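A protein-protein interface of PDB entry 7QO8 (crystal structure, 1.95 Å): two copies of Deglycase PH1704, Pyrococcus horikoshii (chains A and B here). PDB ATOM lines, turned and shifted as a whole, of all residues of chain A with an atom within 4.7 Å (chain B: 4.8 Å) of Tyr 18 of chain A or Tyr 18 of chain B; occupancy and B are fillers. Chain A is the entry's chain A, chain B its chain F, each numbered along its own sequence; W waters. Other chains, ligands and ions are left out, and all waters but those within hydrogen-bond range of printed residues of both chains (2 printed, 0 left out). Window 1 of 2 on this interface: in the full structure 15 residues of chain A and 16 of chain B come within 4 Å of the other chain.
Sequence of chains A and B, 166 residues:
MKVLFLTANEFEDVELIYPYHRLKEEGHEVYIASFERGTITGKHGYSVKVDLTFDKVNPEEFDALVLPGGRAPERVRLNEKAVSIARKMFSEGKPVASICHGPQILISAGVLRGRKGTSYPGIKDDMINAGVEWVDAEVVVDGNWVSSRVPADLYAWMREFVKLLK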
ATOM      1  N   VAL A  14     -21.196  36.424  21.350  1.00  0.00           N
ATOM      2  CA  VAL A  14     -20.755  35.304  22.193  1.00  0.00           C
ATOM      3  C   VAL A  14     -21.802  34.919  23.233  1.00  0.00           C
ATOM      4  O   VAL A  14     -21.821  33.774  23.698  1.00  0.00           O
ATOM      5  CB  VAL A  14     -19.397  35.588  22.874  1.00  0.00           C
ATOM      6  CG1 VAL A  14     -18.281  35.689  21.824  1.00  0.00           C
ATOM      7  CG2 VAL A  14     -19.451  36.845  23.729  1.00  0.00           C
ATOM      8  N   GLU A  15     -22.691  35.843  23.603  1.00  0.00           N
ATOM      9  CA  GLU A  15     -23.723  35.501  24.570  1.00  0.00           C
ATOM     10  C   GLU A  15     -24.752  34.555  23.979  1.00  0.00           C
ATOM     11  O   GLU A  15     -25.466  33.879  24.739  1.00  0.00           O
ATOM     12  CB  GLU A  15     -24.404  36.782  25.093  1.00  0.00           C
ATOM     13  CG  GLU A  15     -23.481  37.566  25.974  1.00  0.00           C
ATOM     14  CD  GLU A  15     -24.028  38.929  26.335  1.00  0.00           C
ATOM     15  OE1 GLU A  15     -25.199  39.206  26.038  1.00  0.00           O
ATOM     16  OE2 GLU A  15     -23.251  39.718  26.896  1.00  0.00           O
ATOM     17  N   LEU A  16     -24.822  34.462  22.649  1.00  0.00           N
ATOM     18  CA  LEU A  16     -25.649  33.443  22.023  1.00  0.00           C
ATOM     19  C   LEU A  16     -24.837  32.189  21.725  1.00  0.00           C
ATOM     20  O   LEU A  16     -25.238  31.086  22.098  1.00  0.00           O
ATOM     21  CB  LEU A  16     -26.272  33.990  20.735  1.00  0.00           C
ATOM     22  CG  LEU A  16     -27.073  33.040  19.840  1.00  0.00           C
ATOM     23  CD1 LEU A  16     -27.964  32.184  20.671  1.00  0.00           C
ATOM     24  CD2 LEU A  16     -27.919  33.862  18.882  1.00  0.00           C
ATOM     25  N   ILE A  17     -23.675  32.360  21.098  1.00  0.00           N
ATOM     26  CA  ILE A  17     -22.912  31.220  20.600  1.00  0.00           C
ATOM     27  C   ILE A  17     -22.362  30.398  21.756  1.00  0.00           C
ATOM     28  O   ILE A  17     -22.362  29.167  21.700  1.00  0.00           O
ATOM     29  CB  ILE A  17     -21.804  31.716  19.649  1.00  0.00           C
ATOM     30  CG1 ILE A  17     -22.458  32.332  18.393  1.00  0.00           C
ATOM     31  CG2 ILE A  17     -20.831  30.582  19.311  1.00  0.00           C
ATOM     32  CD1 ILE A  17     -21.526  33.211  17.537  1.00  0.00           C
ATOM     33  N   TYR A  18     -21.929  31.050  22.845  1.00  0.00           N
ATOM     34  CA  TYR A  18     -21.355  30.276  23.946  1.00  0.00           C
ATOM     35  C   TYR A  18     -22.354  29.296  24.549  1.00  0.00           C
ATOM     36  O   TYR A  18     -22.085  28.082  24.528  1.00  0.00           O
ATOM     37  CB  TYR A  18     -20.763  31.199  25.023  1.00  0.00           C
ATOM     38  CG  TYR A  18     -20.062  30.401  26.100  1.00  0.00           C
ATOM     39  CD1 TYR A  18     -18.772  29.919  25.899  1.00  0.00           C
ATOM     40  CD2 TYR A  18     -20.708  30.067  27.289  1.00  0.00           C
ATOM     41  CE1 TYR A  18     -18.126  29.161  26.866  1.00  0.00           C
ATOM     42  CE2 TYR A  18     -20.072  29.309  28.271  1.00  0.00           C
ATOM     43  CZ  TYR A  18     -18.776  28.852  28.040  1.00  0.00           C
ATOM     44  OH  TYR A  18     -18.123  28.106  28.987  1.00  0.00           O
ATOM     45  N   PRO A  19     -23.512  29.726  25.081  1.00  0.00           N
ATOM     46  CA  PRO A  19     -24.432  28.733  25.664  1.00  0.00           C
ATOM     47  C   PRO A  19     -24.987  27.765  24.636  1.00  0.00           C
ATOM     48  O   PRO A  19     -25.285  26.618  24.987  1.00  0.00           O
ATOM     49  CB  PRO A  19     -25.540  29.599  26.289  1.00  0.00           C
ATOM     50  CG  PRO A  19     -25.538  30.856  25.456  1.00  0.00           C
ATOM     51  CD  PRO A  19     -24.065  31.097  25.181  1.00  0.00           C
ATOM     52  N   TYR A  20     -25.153  28.201  23.386  1.00  0.00           N
ATOM     53  CA  TYR A  20     -25.579  27.293  22.320  1.00  0.00           C
ATOM     54  C   TYR A  20     -24.684  26.051  22.250  1.00  0.00           C
ATOM     55  O   TYR A  20     -25.162  24.916  22.328  1.00  0.00           O
ATOM     56  CB  TYR A  20     -25.578  28.035  20.982  1.00  0.00           C
ATOM     57  CG  TYR A  20     -26.142  27.225  19.844  1.00  0.00           C
ATOM     58  CD1 TYR A  20     -27.477  27.333  19.489  1.00  0.00           C
ATOM     59  CD2 TYR A  20     -25.338  26.348  19.115  1.00  0.00           C
ATOM     60  CE1 TYR A  20     -28.004  26.588  18.444  1.00  0.00           C
ATOM     61  CE2 TYR A  20     -25.853  25.606  18.075  1.00  0.00           C
ATOM     62  CZ  TYR A  20     -27.186  25.727  17.744  1.00  0.00           C
ATOM     63  OH  TYR A  20     -27.703  24.981  16.712  1.00  0.00           O
ATOM     64  N   HIS A  21     -23.371  26.251  22.147  1.00  0.00           N
ATOM     65  CA  HIS A  21     -22.466  25.111  22.059  1.00  0.00           C
ATOM     66  C   HIS A  21     -22.283  24.437  23.409  1.00  0.00           C
ATOM     67  O   HIS A  21     -22.212  23.204  23.473  1.00  0.00           O
ATOM     68  CB  HIS A  21     -21.114  25.552  21.490  1.00  0.00           C
ATOM     69  CG  HIS A  21     -21.159  25.810  20.024  1.00  0.00           C
ATOM     70  ND1 HIS A  21     -21.009  24.805  19.089  1.00  0.00           N
ATOM     71  CD2 HIS A  21     -21.384  26.947  19.326  1.00  0.00           C
ATOM     72  CE1 HIS A  21     -21.131  25.318  17.879  1.00  0.00           C
ATOM     73  NE2 HIS A  21     -21.368  26.614  17.995  1.00  0.00           N
ATOM     74  N   ARG A  22     -22.249  25.221  24.501  1.00  0.00           N
ATOM     75  CA  ARG A  22     -22.064  24.625  25.823  1.00  0.00           C
ATOM     76  C   ARG A  22     -23.179  23.640  26.140  1.00  0.00           C
ATOM     77  O   ARG A  22     -22.925  22.548  26.673  1.00  0.00           O
ATOM     78  CB  ARG A  22     -21.991  25.709  26.908  1.00  0.00           C
ATOM     79  CG  ARG A  22     -21.799  25.145  28.338  1.00  0.00           C
ATOM     80  CD  ARG A  22     -20.476  24.354  28.462  1.00  0.00           C
ATOM     81  NE  ARG A  22     -20.335  23.740  29.787  1.00  0.00           N
ATOM     82  CZ  ARG A  22     -20.705  22.495  30.072  1.00  0.00           C
ATOM     83  NH1 ARG A  22     -21.238  21.737  29.125  1.00  0.00           N
ATOM     84  NH2 ARG A  22     -20.552  22.008  31.300  1.00  0.00           N
ATOM     85  N   GLU A  25     -22.989  20.493  24.007  1.00  0.00           N
ATOM     86  CA  GLU A  25     -21.997  19.574  24.538  1.00  0.00           C
ATOM     87  C   GLU A  25     -22.632  18.560  25.478  1.00  0.00           C
ATOM     88  O   GLU A  25     -22.284  17.372  25.442  1.00  0.00           O
ATOM     89  CB  GLU A  25     -20.890  20.340  25.261  1.00  0.00           C
ATOM     90  CG  GLU A  25     -20.068  19.412  26.123  1.00  0.00           C
ATOM     91  CD  GLU A  25     -19.016  20.115  26.944  1.00  0.00           C
ATOM     92  OE1 GLU A  25     -18.749  21.312  26.687  1.00  0.00           O
ATOM     93  OE2 GLU A  25     -18.443  19.442  27.840  1.00  0.00           O
ATOM     94  N   LEU A 154     -19.214  34.563  31.141  1.00  0.00           N
ATOM     95  CA  LEU A 154     -19.786  33.392  30.477  1.00  0.00           C
ATOM     96  C   LEU A 154     -19.470  32.098  31.213  1.00  0.00           C
ATOM     97  O   LEU A 154     -20.357  31.258  31.417  1.00  0.00           O
ATOM     98  CB  LEU A 154     -19.297  33.300  29.027  1.00  0.00           C
ATOM     99  CG  LEU A 154     -19.895  34.351  28.099  1.00  0.00           C
ATOM    100  CD1 LEU A 154     -19.089  34.393  26.802  1.00  0.00           C
ATOM    101  CD2 LEU A 154     -21.385  34.097  27.845  1.00  0.00           C
ATOM    102  N   TYR A 155     -18.217  31.928  31.637  1.00  0.00           N
ATOM    103  CA  TYR A 155     -17.827  30.670  32.258  1.00  0.00           C
ATOM    104  C   TYR A 155     -18.680  30.376  33.492  1.00  0.00           C
ATOM    105  O   TYR A 155     -19.203  29.266  33.640  1.00  0.00           O
ATOM    106  CB  TYR A 155     -16.338  30.709  32.613  1.00  0.00           C
ATOM    107  CG  TYR A 155     -16.005  31.548  33.842  1.00  0.00           C
ATOM    108  CD1 TYR A 155     -15.680  30.927  35.058  1.00  0.00           C
ATOM    109  CD2 TYR A 155     -16.014  32.937  33.794  1.00  0.00           C
ATOM    110  CE1 TYR A 155     -15.370  31.661  36.181  1.00  0.00           C
ATOM    111  CE2 TYR A 155     -15.699  33.700  34.940  1.00  0.00           C
ATOM    112  CZ  TYR A 155     -15.389  33.042  36.124  1.00  0.00           C
ATOM    113  OH  TYR A 155     -15.076  33.743  37.260  1.00  0.00           O
ATOM    114  N   MET A 158     -22.781  29.693  32.537  1.00  0.00           N
ATOM    115  CA  MET A 158     -23.198  28.364  32.117  1.00  0.00           C
ATOM    116  C   MET A 158     -22.765  27.294  33.106  1.00  0.00           C
ATOM    117  O   MET A 158     -23.425  26.253  33.189  1.00  0.00           O
ATOM    118  CB  MET A 158     -22.677  28.062  30.704  1.00  0.00           C
ATOM    119  CG  MET A 158     -23.540  28.752  29.624  1.00  0.00           C
ATOM    120  SD  MET A 158     -25.247  28.152  29.631  1.00  0.00           S
ATOM    121  CE  MET A 158     -26.176  29.624  30.184  1.00  0.00           C
ATOM    122  N   ASP B  13     -12.744  34.927  16.640  1.00  0.00           N
ATOM    123  CA  ASP B  13     -13.126  35.371  17.984  1.00  0.00           C
ATOM    124  C   ASP B  13     -13.672  34.229  18.820  1.00  0.00           C
ATOM    125  O   ASP B  13     -13.222  34.005  19.960  1.00  0.00           O
ATOM    126  CB  ASP B  13     -14.153  36.513  17.910  1.00  0.00           C
ATOM    127  CG  ASP B  13     -13.662  37.682  17.063  1.00  0.00           C
ATOM    128  OD1 ASP B  13     -13.604  38.802  17.594  1.00  0.00           O
ATOM    129  OD2 ASP B  13     -13.307  37.468  15.887  1.00  0.00           O
ATOM    130  N   VAL B  14     -14.669  33.513  18.293  1.00  0.00           N
ATOM    131  CA  VAL B  14     -15.301  32.501  19.128  1.00  0.00           C
ATOM    132  C   VAL B  14     -14.382  31.314  19.324  1.00  0.00           C
ATOM    133  O   VAL B  14     -14.500  30.596  20.318  1.00  0.00           O
ATOM    134  CB  VAL B  14     -16.672  32.085  18.566  1.00  0.00           C
ATOM    135  CG1 VAL B  14     -17.597  33.280  18.548  1.00  0.00           C
ATOM    136  CG2 VAL B  14     -16.557  31.448  17.167  1.00  0.00           C
ATOM    137  N   GLU B  15     -13.435  31.090  18.411  1.00  0.00           N
ATOM    138  CA  GLU B  15     -12.538  29.956  18.610  1.00  0.00           C
ATOM    139  C   GLU B  15     -11.556  30.197  19.738  1.00  0.00           C
ATOM    140  O   GLU B  15     -10.978  29.233  20.244  1.00  0.00           O
ATOM    141  CB  GLU B  15     -11.794  29.630  17.313  1.00  0.00           C
ATOM    142  CG  GLU B  15     -12.715  29.115  16.251  1.00  0.00           C
ATOM    143  CD  GLU B  15     -12.014  28.911  14.908  1.00  0.00           C
ATOM    144  OE1 GLU B  15     -10.780  29.096  14.837  1.00  0.00           O
ATOM    145  OE2 GLU B  15     -12.716  28.605  13.928  1.00  0.00           O
ATOM    146  N   LEU B  16     -11.355  31.454  20.140  1.00  0.00           N
ATOM    147  CA  LEU B  16     -10.598  31.750  21.353  1.00  0.00           C
ATOM    148  C   LEU B  16     -11.520  31.886  22.564  1.00  0.00           C
ATOM    149  O   LEU B  16     -11.255  31.307  23.626  1.00  0.00           O
ATOM    150  CB  LEU B  16      -9.765  33.018  21.149  1.00  0.00           C
ATOM    151  CG  LEU B  16      -9.047  33.737  22.291  1.00  0.00           C
ATOM    152  CD1 LEU B  16      -8.418  32.762  23.213  1.00  0.00           C
ATOM    153  CD2 LEU B  16      -7.980  34.653  21.717  1.00  0.00           C
ATOM    154  N   ILE B  17     -12.616  32.637  22.415  1.00  0.00           N
ATOM    155  CA  ILE B  17     -13.434  32.968  23.577  1.00  0.00           C
ATOM    156  C   ILE B  17     -14.133  31.726  24.122  1.00  0.00           C
ATOM    157  O   ILE B  17     -14.225  31.540  25.336  1.00  0.00           O
ATOM    158  CB  ILE B  17     -14.415  34.100  23.213  1.00  0.00           C
ATOM    159  CG1 ILE B  17     -13.624  35.400  23.042  1.00  0.00           C
ATOM    160  CG2 ILE B  17     -15.499  34.269  24.302  1.00  0.00           C
ATOM    161  CD1 ILE B  17     -14.350  36.507  22.222  1.00  0.00           C
ATOM    162  N   TYR B  18     -14.582  30.817  23.239  1.00  0.00           N
ATOM    163  CA  TYR B  18     -15.302  29.637  23.722  1.00  0.00           C
ATOM    164  C   TYR B  18     -14.439  28.732  24.590  1.00  0.00           C
ATOM    165  O   TYR B  18     -14.818  28.477  25.746  1.00  0.00           O
ATOM    166  CB  TYR B  18     -15.934  28.874  22.551  1.00  0.00           C
ATOM    167  CG  TYR B  18     -16.764  27.713  23.026  1.00  0.00           C
ATOM    168  CD1 TYR B  18     -18.088  27.899  23.390  1.00  0.00           C
ATOM    169  CD2 TYR B  18     -16.220  26.435  23.147  1.00  0.00           C
ATOM    170  CE1 TYR B  18     -18.861  26.867  23.852  1.00  0.00           C
ATOM    171  CE2 TYR B  18     -16.994  25.375  23.609  1.00  0.00           C
ATOM    172  CZ  TYR B  18     -18.325  25.603  23.967  1.00  0.00           C
ATOM    173  OH  TYR B  18     -19.134  24.583  24.435  1.00  0.00           O
ATOM    174  N   PRO B  19     -13.293  28.205  24.119  1.00  0.00           N
ATOM    175  CA  PRO B  19     -12.498  27.349  25.014  1.00  0.00           C
ATOM    176  C   PRO B  19     -11.976  28.091  26.234  1.00  0.00           C
ATOM    177  O   PRO B  19     -11.841  27.477  27.298  1.00  0.00           O
ATOM    178  CB  PRO B  19     -11.345  26.858  24.113  1.00  0.00           C
ATOM    179  CG  PRO B  19     -11.239  27.895  23.040  1.00  0.00           C
ATOM    180  CD  PRO B  19     -12.675  28.292  22.779  1.00  0.00           C
ATOM    181  N   TYR B  20     -11.678  29.388  26.107  1.00  0.00           N
ATOM    182  CA  TYR B  20     -11.268  30.188  27.268  1.00  0.00           C
ATOM    183  C   TYR B  20     -12.269  30.059  28.418  1.00  0.00           C
ATOM    184  O   TYR B  20     -11.909  29.701  29.545  1.00  0.00           O
ATOM    185  CB  TYR B  20     -11.120  31.663  26.854  1.00  0.00           C
ATOM    186  CG  TYR B  20     -10.546  32.560  27.934  1.00  0.00           C
ATOM    187  CD1 TYR B  20      -9.179  32.770  28.022  1.00  0.00           C
ATOM    188  CD2 TYR B  20     -11.366  33.178  28.874  1.00  0.00           C
ATOM    189  CE1 TYR B  20      -8.634  33.592  29.011  1.00  0.00           C
ATOM    190  CE2 TYR B  20     -10.831  33.989  29.876  1.00  0.00           C
ATOM    191  CZ  TYR B  20      -9.460  34.192  29.932  1.00  0.00           C
ATOM    192  OH  TYR B  20      -8.901  34.986  30.913  1.00  0.00           O
ATOM    193  N   HIS B  21     -13.545  30.314  28.143  1.00  0.00           N
ATOM    194  CA  HIS B  21     -14.548  30.233  29.207  1.00  0.00           C
ATOM    195  C   HIS B  21     -14.894  28.790  29.556  1.00  0.00           C
ATOM    196  O   HIS B  21     -15.121  28.475  30.731  1.00  0.00           O
ATOM    197  CB  HIS B  21     -15.805  31.009  28.814  1.00  0.00           C
ATOM    198  CG  HIS B  21     -15.623  32.487  28.892  1.00  0.00           C
ATOM    199  ND1 HIS B  21     -15.771  33.191  30.069  1.00  0.00           N
ATOM    200  CD2 HIS B  21     -15.238  33.387  27.959  1.00  0.00           C
ATOM    201  CE1 HIS B  21     -15.517  34.468  29.848  1.00  0.00           C
ATOM    202  NE2 HIS B  21     -15.190  34.612  28.575  1.00  0.00           N
ATOM    203  N   ARG B  22     -14.931  27.904  28.554  1.00  0.00           N
ATOM    204  CA  ARG B  22     -15.242  26.505  28.817  1.00  0.00           C
ATOM    205  C   ARG B  22     -14.218  25.889  29.760  1.00  0.00           C
ATOM    206  O   ARG B  22     -14.565  25.080  30.630  1.00  0.00           O
ATOM    207  CB  ARG B  22     -15.315  25.730  27.495  1.00  0.00           C
ATOM    208  CG  ARG B  22     -15.639  24.243  27.658  1.00  0.00           C
ATOM    209  CD  ARG B  22     -17.015  24.074  28.287  1.00  0.00           C
ATOM    210  NE  ARG B  22     -17.338  22.695  28.640  1.00  0.00           N
ATOM    211  CZ  ARG B  22     -17.091  22.136  29.824  1.00  0.00           C
ATOM    212  NH1 ARG B  22     -16.503  22.828  30.792  1.00  0.00           N
ATOM    213  NH2 ARG B  22     -17.443  20.869  30.033  1.00  0.00           N
ATOM    214  N   GLU B  25     -14.646  27.294  33.303  1.00  0.00           N
ATOM    215  CA  GLU B  25     -15.755  26.668  34.012  1.00  0.00           C
ATOM    216  C   GLU B  25     -15.274  25.478  34.829  1.00  0.00           C
ATOM    217  O   GLU B  25     -15.747  25.247  35.948  1.00  0.00           O
ATOM    218  CB  GLU B  25     -16.843  26.230  33.031  1.00  0.00           C
ATOM    219  CG  GLU B  25     -17.815  25.277  33.692  1.00  0.00           C
ATOM    220  CD  GLU B  25     -18.867  24.729  32.765  1.00  0.00           C
ATOM    221  OE1 GLU B  25     -19.097  25.334  31.690  1.00  0.00           O
ATOM    222  OE2 GLU B  25     -19.466  23.693  33.143  1.00  0.00           O
ATOM    223  N   LEU B 154     -17.616  23.729  17.736  1.00  0.00           N
ATOM    224  CA  LEU B 154     -17.092  24.102  19.057  1.00  0.00           C
ATOM    225  C   LEU B 154     -17.561  23.154  20.159  1.00  0.00           C
ATOM    226  O   LEU B 154     -16.760  22.712  20.992  1.00  0.00           O
ATOM    227  CB  LEU B 154     -17.485  25.545  19.405  1.00  0.00           C
ATOM    228  CG  LEU B 154     -16.685  26.648  18.704  1.00  0.00           C
ATOM    229  CD1 LEU B 154     -17.389  27.985  18.913  1.00  0.00           C
ATOM    230  CD2 LEU B 154     -15.231  26.681  19.171  1.00  0.00           C
ATOM    231  N   TYR B 155     -18.860  22.820  20.171  1.00  0.00           N
ATOM    232  CA  TYR B 155     -19.392  21.978  21.239  1.00  0.00           C
ATOM    233  C   TYR B 155     -18.657  20.639  21.315  1.00  0.00           C
ATOM    234  O   TYR B 155     -18.335  20.167  22.413  1.00  0.00           O
ATOM    235  CB  TYR B 155     -20.894  21.758  21.031  1.00  0.00           C
ATOM    236  CG  TYR B 155     -21.231  20.753  19.929  1.00  0.00           C
ATOM    237  CD1 TYR B 155     -21.656  19.463  20.242  1.00  0.00           C
ATOM    238  CD2 TYR B 155     -21.112  21.094  18.583  1.00  0.00           C
ATOM    239  CE1 TYR B 155     -21.968  18.533  19.235  1.00  0.00           C
ATOM    240  CE2 TYR B 155     -21.421  20.169  17.564  1.00  0.00           C
ATOM    241  CZ  TYR B 155     -21.844  18.894  17.902  1.00  0.00           C
ATOM    242  OH  TYR B 155     -22.136  17.976  16.915  1.00  0.00           O
ATOM    243  N   MET B 158     -14.554  20.979  22.453  1.00  0.00           N
ATOM    244  CA  MET B 158     -14.240  21.066  23.874  1.00  0.00           C
ATOM    245  C   MET B 158     -14.845  19.918  24.679  1.00  0.00           C
ATOM    246  O   MET B 158     -14.320  19.584  25.747  1.00  0.00           O
ATOM    247  CB  MET B 158     -14.701  22.413  24.436  1.00  0.00           C
ATOM    248  CG  MET B 158     -13.736  23.567  24.124  1.00  0.00           C
ATOM    249  SD  MET B 158     -12.037  23.340  24.729  1.00  0.00           S
ATOM    250  CE  MET B 158     -11.136  23.054  23.159  1.00  0.00           C
HETATM  251  O   HOH W   1     -19.332  27.689  31.151  1.00  0.00           O
HETATM  252  O   HOH W   2     -17.959  22.156  24.568  1.00  0.00           O
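The side-chain carboxylate (OE2) of Glu 25 of chain B lies within salt-bridge range of the guanidinium group (NH2) of Arg 22 of chain A. O of His 21 of chain B lies close to OH of Tyr 18 of chain A. The guanidinium group (NE) of Arg 22 of chain B sits close to the guanidinium group (NE) of Arg 22 of chain A (3.4 Å). A ring nitrogen (ND1) of His 21 of chain B is in hydrogen-bond range of the backbone NH (N) of Tyr 155 of chain A (3.2 Å). ND1 of His 21 of chain A is in hydrogen-bond range of N of Tyr 155 of chain B (3.1 Å). OE1 of Glu 25 of chain A is in salt-bridge range of NE of Arg 22 of chain B (2.8 Å). The backbone NH (N) of Arg 22 of chain B lies within hydrogen-bond range of the side-chain hydroxyl (OH) of Tyr 18 of chain A (3.2 Å). OH of Tyr 18 of chain B is in hydrogen-bond range of N of Arg 22 of chain A (3.2 Å).
The guanidinium group (NH1) of Arg 22 of chain B is in salt-bridge range of the side-chain carboxylate (OE1) of Glu 25 of chain B (3.7 Å). NH1 of Arg 22 of chain A is in salt-bridge range of OE1 of Glu 25 of chain A (3.5 Å).
Among the printed residues, pairs that only touch across the chains: Val 14 of chain A with Ile 17 of chain B, Tyr 18 of chain A with Tyr 18 of chain B, Tyr 18 of chain A with Glu 25 of chain B, His 21 of chain A with Tyr 18 of chain B, His 21 of chain A with Leu 154 of chain B, Glu 25 of chain A with Tyr 18 of chain B, Glu 25 of chain A with Tyr 155 of chain B, Leu 154 of chain A with His 21 of chain B and Tyr 155 of chain A with Glu 25 of chain B.
Printed residues of chain B within 4 Å of Tyr 18 of chain A: Tyr 18 (3.3 Å), His 21 (3.3 Å), Arg 22 (3.2 Å) and Glu 25 (3.99 Å). Printed residues of chain A within 4 Å of Tyr 18 of chain B: Tyr 18 (3.3 Å), His 21 (3.3 Å), Arg 22 (3.2 Å) and Glu 25 (3.99 Å). Of the printed residues of chain A, Glu 25 of chain B touches Tyr 18 (3.99 Å), Arg 22 (2.7 Å) and Tyr 155 (3.9 Å). Of the printed residues of chain B, Tyr 155 of chain A touches His 21 (3.2 Å) and Glu 25 (3.9 Å). Of the printed residues of chain A, Ile 17 of chain B touches Val 14. Printed residues of chain B within 4 Å of Arg 22 of chain A: Tyr 18, Arg 22 and Glu 25. Of the printed residues of chain B, Leu 154 of chain A touches His 21. The nearest printed residue of chain B that does not touch Tyr 18 of chain A is Ile 17 of chain B (4.8 Å). The nearest printed residue of chain A that does not touch Tyr 18 of chain B is Ile 17 of chain A (4.7 Å).
Of the 13 printed residues of chain A, 7 touch a printed residue of chain B. Of the 14 printed residues of chain B, 7 touch a printed residue of chain A. Hydrophobic or aromatic side chains of chain B that line the printed part of chain A: Ile 17, Tyr 18, His 21, Leu 154 and Tyr 155. Among the printed residues, 17 pairs touch across the chains. Among the printed residues, Asp or Glu carboxylates within 4 Å of a Lys or Arg side-chain nitrogen of the other chain: Arg 22 of chain A with Glu 25 of chain B (2.7 Å) and Glu 25 of chain A with Arg 22 of chain B (2.8 Å).
Tyr 18 of chain A touches its own counterpart, Tyr 18 of chain B. Tyr 18 of chain A touches Arg 22 of chain B, and with the chains exchanged Arg 22 of chain A touches Tyr 18 of chain B. Arg 22 of chain B touches its own counterpart, Arg 22 of chain A. Arg 22 of chain A touches Glu 25 of chain B, and with the chains exchanged Glu 25 of chain A touches Arg 22 of chain B.
Water W2 lies within hydrogen-bond range of the side-chain carboxylate of Glu 25 of chain A, the side-chain hydroxyl of Tyr 18 of chain B and the backbone carbonyl oxygen of Tyr 155 of chain B. Water W1 lies within hydrogen-bond range of OE1 of Glu 25 of chain B (2.4 Å), OH of Tyr 18 of chain A (2.5 Å) and O of Tyr 155 of chain A (2.9 Å).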
